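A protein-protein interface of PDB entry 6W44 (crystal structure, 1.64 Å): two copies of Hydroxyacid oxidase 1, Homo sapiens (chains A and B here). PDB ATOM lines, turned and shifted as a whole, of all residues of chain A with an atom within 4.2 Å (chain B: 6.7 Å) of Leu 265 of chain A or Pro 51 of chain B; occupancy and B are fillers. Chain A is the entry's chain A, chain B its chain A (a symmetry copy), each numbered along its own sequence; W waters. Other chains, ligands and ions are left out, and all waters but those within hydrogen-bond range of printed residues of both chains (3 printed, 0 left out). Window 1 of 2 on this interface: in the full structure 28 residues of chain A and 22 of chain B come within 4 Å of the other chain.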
ATOM      1  N   LEU A 239      23.222  18.352 -20.914  1.00  0.00           N
ATOM      2  CA  LEU A 239      22.705  19.355 -21.851  1.00  0.00           C
ATOM      3  C   LEU A 239      23.201  20.763 -21.521  1.00  0.00           C
ATOM      4  O   LEU A 239      22.977  21.635 -22.361  1.00  0.00           O
ATOM      5  CB  LEU A 239      21.173  19.324 -21.928  1.00  0.00           C
ATOM      6  CG  LEU A 239      20.589  18.023 -22.460  1.00  0.00           C
ATOM      7  CD1 LEU A 239      19.076  17.976 -22.258  1.00  0.00           C
ATOM      8  CD2 LEU A 239      20.957  17.869 -23.926  1.00  0.00           C
ATOM      9  N   ARG A 240      23.893  20.968 -20.424  1.00  0.00           N
ATOM     10  CA  ARG A 240      24.344  22.313 -20.015  1.00  0.00           C
ATOM     11  C   ARG A 240      25.867  22.351 -19.889  1.00  0.00           C
ATOM     12  O   ARG A 240      26.453  21.406 -19.372  1.00  0.00           O
ATOM     13  CB  ARG A 240      23.772  22.697 -18.649  1.00  0.00           C
ATOM     14  CG  ARG A 240      22.270  22.928 -18.561  1.00  0.00           C
ATOM     15  CD  ARG A 240      21.850  23.068 -17.118  1.00  0.00           C
ATOM     16  NE  ARG A 240      22.389  24.259 -16.469  1.00  0.00           N
ATOM     17  CZ  ARG A 240      21.712  25.376 -16.174  1.00  0.00           C
ATOM     18  NH1 ARG A 240      22.325  26.371 -15.538  1.00  0.00           N
ATOM     19  NH2 ARG A 240      20.446  25.511 -16.500  1.00  0.00           N
ATOM     20  N   ASP A 243      27.084  21.889 -16.143  1.00  0.00           N
ATOM     21  CA  ASP A 243      27.118  20.481 -15.764  1.00  0.00           C
ATOM     22  C   ASP A 243      28.288  19.767 -16.434  1.00  0.00           C
ATOM     23  O   ASP A 243      28.895  18.908 -15.800  1.00  0.00           O
ATOM     24  CB  ASP A 243      25.812  19.777 -16.134  1.00  0.00           C
ATOM     25  CG  ASP A 243      24.666  20.036 -15.171  1.00  0.00           C
ATOM     26  OD1 ASP A 243      24.887  20.806 -14.166  1.00  0.00           O
ATOM     27  OD2 ASP A 243      23.529  19.529 -15.471  1.00  0.00           O
ATOM     28  N   GLN A 264      12.758  11.932 -22.306  1.00  0.00           N
ATOM     29  CA  GLN A 264      12.794  12.331 -20.873  1.00  0.00           C
ATOM     30  C   GLN A 264      12.031  13.659 -20.763  1.00  0.00           C
ATOM     31  O   GLN A 264      10.806  13.633 -20.674  1.00  0.00           O
ATOM     32  CB  GLN A 264      14.238  12.341 -20.356  1.00  0.00           C
ATOM     33  CG  GLN A 264      14.757  10.920 -20.144  1.00  0.00           C
ATOM     34  CD  GLN A 264      13.985  10.213 -19.049  1.00  0.00           C
ATOM     35  OE1 GLN A 264      13.212   9.284 -19.326  1.00  0.00           O
ATOM     36  NE2 GLN A 264      14.104  10.718 -17.830  1.00  0.00           N
ATOM     37  N   LEU A 265      12.734  14.778 -20.676  1.00  0.00           N
ATOM     38  CA  LEU A 265      12.075  16.099 -20.585  1.00  0.00           C
ATOM     39  C   LEU A 265      11.823  16.619 -21.998  1.00  0.00           C
ATOM     40  O   LEU A 265      12.783  16.839 -22.743  1.00  0.00           O
ATOM     41  CB  LEU A 265      12.991  17.022 -19.798  1.00  0.00           C
ATOM     42  CG  LEU A 265      12.473  18.432 -19.551  1.00  0.00           C
ATOM     43  CD1 LEU A 265      11.196  18.391 -18.755  1.00  0.00           C
ATOM     44  CD2 LEU A 265      13.540  19.243 -18.796  1.00  0.00           C
ATOM     45  N   ASP A 266      10.549  16.797 -22.372  1.00  0.00           N
ATOM     46  CA  ASP A 266      10.223  17.421 -23.677  1.00  0.00           C
ATOM     47  C   ASP A 266      10.434  18.923 -23.604  1.00  0.00           C
ATOM     48  O   ASP A 266      10.116  19.521 -22.588  1.00  0.00           O
ATOM     49  CB  ASP A 266       8.816  17.094 -24.152  1.00  0.00           C
ATOM     50  CG  ASP A 266       8.669  17.339 -25.630  1.00  0.00           C
ATOM     51  OD1 ASP A 266       9.626  17.019 -26.377  1.00  0.00           O
ATOM     52  OD2 ASP A 266       7.623  17.850 -26.043  1.00  0.00           O
ATOM     53  N   GLY A 267      10.912  19.497 -24.702  1.00  0.00           N
ATOM     54  CA  GLY A 267      11.173  20.933 -24.823  1.00  0.00           C
ATOM     55  C   GLY A 267      12.593  21.301 -24.466  1.00  0.00           C
ATOM     56  O   GLY A 267      12.893  22.507 -24.469  1.00  0.00           O
ATOM     57  N   VAL A 268      13.459  20.319 -24.265  1.00  0.00           N
ATOM     58  CA  VAL A 268      14.914  20.596 -24.258  1.00  0.00           C
ATOM     59  C   VAL A 268      15.351  20.810 -25.699  1.00  0.00           C
ATOM     60  O   VAL A 268      14.680  20.406 -26.648  1.00  0.00           O
ATOM     61  CB  VAL A 268      15.701  19.486 -23.567  1.00  0.00           C
ATOM     62  CG1 VAL A 268      15.238  19.303 -22.132  1.00  0.00           C
ATOM     63  CG2 VAL A 268      15.595  18.175 -24.360  1.00  0.00           C
ATOM     64  N   LEU B  49      14.070  24.312 -22.597  1.00  0.00           N
ATOM     65  CA  LEU B  49      14.472  23.990 -21.204  1.00  0.00           C
ATOM     66  C   LEU B  49      15.910  23.495 -21.213  1.00  0.00           C
ATOM     67  O   LEU B  49      16.273  22.703 -22.090  1.00  0.00           O
ATOM     68  CB  LEU B  49      13.567  22.929 -20.588  1.00  0.00           C
ATOM     69  CG  LEU B  49      12.195  23.493 -20.175  1.00  0.00           C
ATOM     70  CD1 LEU B  49      11.184  22.335 -20.056  1.00  0.00           C
ATOM     71  CD2 LEU B  49      12.266  24.335 -18.891  1.00  0.00           C
ATOM     72  N   TYR B  50      16.704  23.955 -20.258  1.00  0.00           N
ATOM     73  CA  TYR B  50      18.120  23.574 -20.056  1.00  0.00           C
ATOM     74  C   TYR B  50      18.250  22.927 -18.692  1.00  0.00           C
ATOM     75  O   TYR B  50      18.570  23.580 -17.685  1.00  0.00           O
ATOM     76  CB  TYR B  50      18.988  24.838 -20.204  1.00  0.00           C
ATOM     77  CG  TYR B  50      19.064  25.303 -21.633  1.00  0.00           C
ATOM     78  CD1 TYR B  50      18.019  26.013 -22.204  1.00  0.00           C
ATOM     79  CD2 TYR B  50      20.141  24.963 -22.432  1.00  0.00           C
ATOM     80  CE1 TYR B  50      18.015  26.304 -23.543  1.00  0.00           C
ATOM     81  CE2 TYR B  50      20.185  25.333 -23.759  1.00  0.00           C
ATOM     82  CZ  TYR B  50      19.112  25.978 -24.310  1.00  0.00           C
ATOM     83  OH  TYR B  50      19.177  26.383 -25.615  1.00  0.00           O
ATOM     84  N   PRO B  51      17.897  21.636 -18.567  1.00  0.00           N
ATOM     85  CA  PRO B  51      17.806  20.968 -17.274  1.00  0.00           C
ATOM     86  C   PRO B  51      19.172  20.761 -16.627  1.00  0.00           C
ATOM     87  O   PRO B  51      20.149  20.452 -17.320  1.00  0.00           O
ATOM     88  CB  PRO B  51      17.181  19.606 -17.596  1.00  0.00           C
ATOM     89  CG  PRO B  51      17.569  19.379 -19.015  1.00  0.00           C
ATOM     90  CD  PRO B  51      17.453  20.746 -19.643  1.00  0.00           C
ATOM     91  N   ARG B  52      19.228  20.922 -15.306  1.00  0.00           N
ATOM     92  CA  ARG B  52      20.420  20.514 -14.525  1.00  0.00           C
ATOM     93  C   ARG B  52      20.260  19.069 -14.065  1.00  0.00           C
ATOM     94  O   ARG B  52      19.141  18.614 -13.660  1.00  0.00           O
ATOM     95  CB  ARG B  52      20.581  21.360 -13.268  1.00  0.00           C
ATOM     96  CG  ARG B  52      20.816  22.828 -13.540  1.00  0.00           C
ATOM     97  CD  ARG B  52      21.142  23.462 -12.176  1.00  0.00           C
ATOM     98  NE  ARG B  52      21.498  24.856 -12.300  1.00  0.00           N
ATOM     99  CZ  ARG B  52      20.609  25.866 -12.409  1.00  0.00           C
ATOM    100  NH1 ARG B  52      21.045  27.117 -12.470  1.00  0.00           N
ATOM    101  NH2 ARG B  52      19.307  25.634 -12.459  1.00  0.00           N
ATOM    102  N   MET B  53      21.338  18.306 -14.151  1.00  0.00           N
ATOM    103  CA  MET B  53      21.345  16.894 -13.746  1.00  0.00           C
ATOM    104  C   MET B  53      21.929  16.744 -12.323  1.00  0.00           C
ATOM    105  O   MET B  53      22.702  17.636 -11.881  1.00  0.00           O
ATOM    106  CB  MET B  53      22.137  16.093 -14.781  1.00  0.00           C
ATOM    107  CG  MET B  53      21.728  16.350 -16.231  1.00  0.00           C
ATOM    108  SD  MET B  53      20.005  15.886 -16.398  1.00  0.00           S
ATOM    109  CE  MET B  53      19.617  16.594 -18.020  1.00  0.00           C
ATOM    110  N   THR B 298       5.381  21.367 -18.331  1.00  0.00           N
ATOM    111  CA  THR B 298       6.547  22.167 -18.783  1.00  0.00           C
ATOM    112  C   THR B 298       6.140  23.619 -19.029  1.00  0.00           C
ATOM    113  O   THR B 298       7.013  24.517 -18.896  1.00  0.00           O
ATOM    114  CB  THR B 298       7.223  21.575 -20.022  1.00  0.00           C
ATOM    115  OG1 THR B 298       6.235  21.267 -21.020  1.00  0.00           O
ATOM    116  CG2 THR B 298       7.970  20.293 -19.693  1.00  0.00           C
ATOM    117  N   LEU B 301       6.514  25.195 -15.663  1.00  0.00           N
ATOM    118  CA  LEU B 301       7.944  25.357 -15.328  1.00  0.00           C
ATOM    119  C   LEU B 301       8.516  26.563 -16.085  1.00  0.00           C
ATOM    120  O   LEU B 301       9.262  27.378 -15.482  1.00  0.00           O
ATOM    121  CB  LEU B 301       8.680  24.053 -15.658  1.00  0.00           C
ATOM    122  CG  LEU B 301      10.166  24.087 -15.361  1.00  0.00           C
ATOM    123  CD1 LEU B 301      10.407  24.355 -13.891  1.00  0.00           C
ATOM    124  CD2 LEU B 301      10.857  22.794 -15.768  1.00  0.00           C
ATOM    125  N   LEU B 342       6.996  16.120 -12.501  1.00  0.00           N
ATOM    126  CA  LEU B 342       7.982  15.425 -13.345  1.00  0.00           C
ATOM    127  C   LEU B 342       8.905  16.440 -14.034  1.00  0.00           C
ATOM    128  O   LEU B 342      10.125  16.218 -14.070  1.00  0.00           O
ATOM    129  CB  LEU B 342       7.287  14.513 -14.360  1.00  0.00           C
ATOM    130  CG  LEU B 342       8.230  13.707 -15.236  1.00  0.00           C
ATOM    131  CD1 LEU B 342       9.113  12.785 -14.376  1.00  0.00           C
ATOM    132  CD2 LEU B 342       7.392  12.924 -16.245  1.00  0.00           C
ATOM    133  N   ALA B 343       8.384  17.528 -14.570  1.00  0.00           N
ATOM    134  CA  ALA B 343       9.217  18.527 -15.267  1.00  0.00           C
ATOM    135  C   ALA B 343      10.193  19.117 -14.268  1.00  0.00           C
ATOM    136  O   ALA B 343      11.364  19.288 -14.625  1.00  0.00           O
ATOM    137  CB  ALA B 343       8.340  19.585 -15.889  1.00  0.00           C
ATOM    138  N   MET B 344       9.743  19.419 -13.049  1.00  0.00           N
ATOM    139  CA  MET B 344      10.654  19.973 -12.007  1.00  0.00           C
ATOM    140  C   MET B 344      11.759  18.946 -11.732  1.00  0.00           C
ATOM    141  O   MET B 344      12.971  19.289 -11.738  1.00  0.00           O
ATOM    142  CB  MET B 344       9.896  20.276 -10.705  1.00  0.00           C
ATOM    143  CG  MET B 344       9.174  21.541 -10.723  1.00  0.00           C
ATOM    144  SD  MET B 344       8.370  21.760  -9.091  1.00  0.00           S
ATOM    145  CE  MET B 344       9.786  21.923  -8.071  1.00  0.00           C
ATOM    146  N   LEU B 346      12.947  16.390 -13.563  1.00  0.00           N
ATOM    147  CA  LEU B 346      13.839  16.122 -14.703  1.00  0.00           C
ATOM    148  C   LEU B 346      14.735  17.333 -14.932  1.00  0.00           C
ATOM    149  O   LEU B 346      15.795  17.133 -15.531  1.00  0.00           O
ATOM    150  CB  LEU B 346      13.043  15.749 -15.949  1.00  0.00           C
ATOM    151  CG  LEU B 346      12.250  14.469 -15.837  1.00  0.00           C
ATOM    152  CD1 LEU B 346      11.589  14.178 -17.178  1.00  0.00           C
ATOM    153  CD2 LEU B 346      13.164  13.324 -15.438  1.00  0.00           C
ATOM    154  N   SER B 347      14.354  18.529 -14.458  1.00  0.00           N
ATOM    155  CA  SER B 347      15.160  19.756 -14.664  1.00  0.00           C
ATOM    156  C   SER B 347      16.052  20.046 -13.459  1.00  0.00           C
ATOM    157  O   SER B 347      16.815  21.045 -13.527  1.00  0.00           O
ATOM    158  CB  SER B 347      14.298  20.930 -14.996  1.00  0.00           C
ATOM    159  OG  SER B 347      13.492  21.294 -13.892  1.00  0.00           O
ATOM    160  N   GLY B 348      15.989  19.206 -12.440  1.00  0.00           N
ATOM    161  CA  GLY B 348      16.867  19.307 -11.272  1.00  0.00           C
ATOM    162  C   GLY B 348      16.348  20.240 -10.219  1.00  0.00           C
ATOM    163  O   GLY B 348      17.172  20.639  -9.333  1.00  0.00           O
ATOM    164  N   THR B 358      18.033  30.561 -15.710  1.00  0.00           N
ATOM    165  CA  THR B 358      18.981  29.831 -16.585  1.00  0.00           C
ATOM    166  C   THR B 358      18.336  28.529 -17.063  1.00  0.00           C
ATOM    167  O   THR B 358      18.865  27.907 -18.026  1.00  0.00           O
ATOM    168  CB  THR B 358      20.313  29.441 -15.931  1.00  0.00           C
ATOM    169  OG1 THR B 358      20.152  28.314 -15.060  1.00  0.00           O
ATOM    170  CG2 THR B 358      20.935  30.627 -15.221  1.00  0.00           C
ATOM    171  N   LEU B 359      17.158  28.207 -16.536  1.00  0.00           N
ATOM    172  CA  LEU B 359      16.493  26.968 -17.050  1.00  0.00           C
ATOM    173  C   LEU B 359      15.933  27.162 -18.438  1.00  0.00           C
ATOM    174  O   LEU B 359      15.533  26.148 -19.045  1.00  0.00           O
ATOM    175  CB  LEU B 359      15.381  26.506 -16.115  1.00  0.00           C
ATOM    176  CG  LEU B 359      15.821  25.917 -14.799  1.00  0.00           C
ATOM    177  CD1 LEU B 359      14.593  25.646 -13.941  1.00  0.00           C
ATOM    178  CD2 LEU B 359      16.609  24.621 -15.015  1.00  0.00           C
HETATM  179  O   HOH W   1       8.259  21.669 -23.485  1.00  0.00           O
HETATM  180  O   HOH W   2      24.061  19.841 -11.716  1.00  0.00           O
HETATM  181  O   HOH W   3      22.684  19.300 -18.097  1.00  0.00           O
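Among the printed residues, merely in contact across the chains: Arg 240 of chain A with Pro 51 of chain B (3.1 Å), Val 268 of chain A with Leu 49 of chain B (3.3 Å), Asp 243 of chain A with Arg 52 of chain B (3.4 Å), Gln 264 of chain A with Leu 346 of chain B (3.6 Å), Val 268 of chain A with Pro 51 of chain B (3.6 Å), Asp 266 of chain A with Thr 298 of chain B (3.7 Å), Leu 265 of chain A with Leu 346 of chain B (3.7 Å), Leu 239 of chain A with Pro 51 of chain B (3.8 Å), Leu 265 of chain A with Pro 51 of chain B (3.9 Å), Leu 265 of chain A with Thr 298 of chain B (3.9 Å), Asp 266 of chain A with Leu 49 of chain B (3.9 Å) and Asp 243 of chain A with Pro 51 of chain B (3.96 Å).
No position is printed for both chains. Of the 17 pairs that touch across the chains among the printed residues, none has its exchanged pair printed and touching as well.
The backbone NH (N) of Arg 52 of chain B is in hydrogen-bond range of the backbone carbonyl oxygen (O) of Ser 347 of chain B (3.0 Å). The guanidinium group (NH1) of Arg 52 of chain B sits at hydrogen-bond distance from the side-chain hydroxyl (OG1) of Thr 358 of chain B. The backbone carbonyl oxygen (O) of Leu 359 of chain B is in hydrogen-bond range of the backbone NH (N) of Tyr 50 of chain B (2.8 Å). The backbone carbonyl oxygen of Arg 52 of chain B lies close to the backbone NH of Gly 348 of chain B (3.4 Å).
Of the printed residues of chain B, Leu 265 of chain A touches Pro 51 (3.9 Å), Thr 298 (3.9 Å) and Leu 346 (3.7 Å). Of the printed residues of chain B, Gly 267 of chain A touches Leu 49. Pro 51 of chain B touches five residues of chain A. Printed residues of chain A within 4 Å of Thr 298 of chain B: Leu 265 (3.9 Å) and Asp 266 (3.7 Å). Printed residues of chain A within 4 Å of Thr 358 of chain B: Arg 240 (3.0 Å). Leu 359 of chain B touches none of the printed residues of chain A. The nearest printed residue of chain B that does not touch Leu 265 of chain A is Ala 343 of chain B (4.01 Å). The nearest printed residue of chain A that does not touch Pro 51 of chain B is Gly 267 of chain A (6.9 Å).
The guanidinium group of Arg 240 of chain A sits at hydrogen-bond distance from the side-chain hydroxyl of Thr 358 of chain B, at 3.0 Å. The guanidinium group of Arg 240 of chain A sits close to the guanidinium group of Arg 52 of chain B (3.4 Å). The backbone carbonyl oxygen (O) of Tyr 50 of chain B sits at hydrogen-bond distance from the guanidinium group (NH2) of Arg 240 of chain A (2.9 Å). The side-chain carboxylate (OD2) of Asp 243 of chain A is in hydrogen-bond range of the backbone NH (N) of Met 53 of chain B. O of Gly 267 of chain A is in hydrogen-bond range of N of Leu 49 of chain B (2.9 Å).
Water W2 bridges O of Met 53 of chain B (2.6 Å) and OD1 of Asp 243 of chain A (2.8 Å). Water W3 lies within hydrogen-bond range of the side-chain carboxylate (OD2) of Asp 243 of chain A, the backbone carbonyl oxygen (O) of Pro 51 of chain B, the backbone NH (N) of Leu 239 of chain A and the backbone NH (N) of Arg 240 of chain A. Water W1 bridges O of Asp 266 of chain A (3.0 Å) and OG1 of Thr 298 of chain B (3.2 Å).
Of the 15 printed residues of chain B, 8 touch a printed residue of chain A. Hydrophobic or aromatic side chains of chain A within 4 Å of the printed part of chain B: Leu 239, Leu 265 and Val 268. Along chain A the printed residues that touch a printed residue of chain B span positions 239 to 268.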
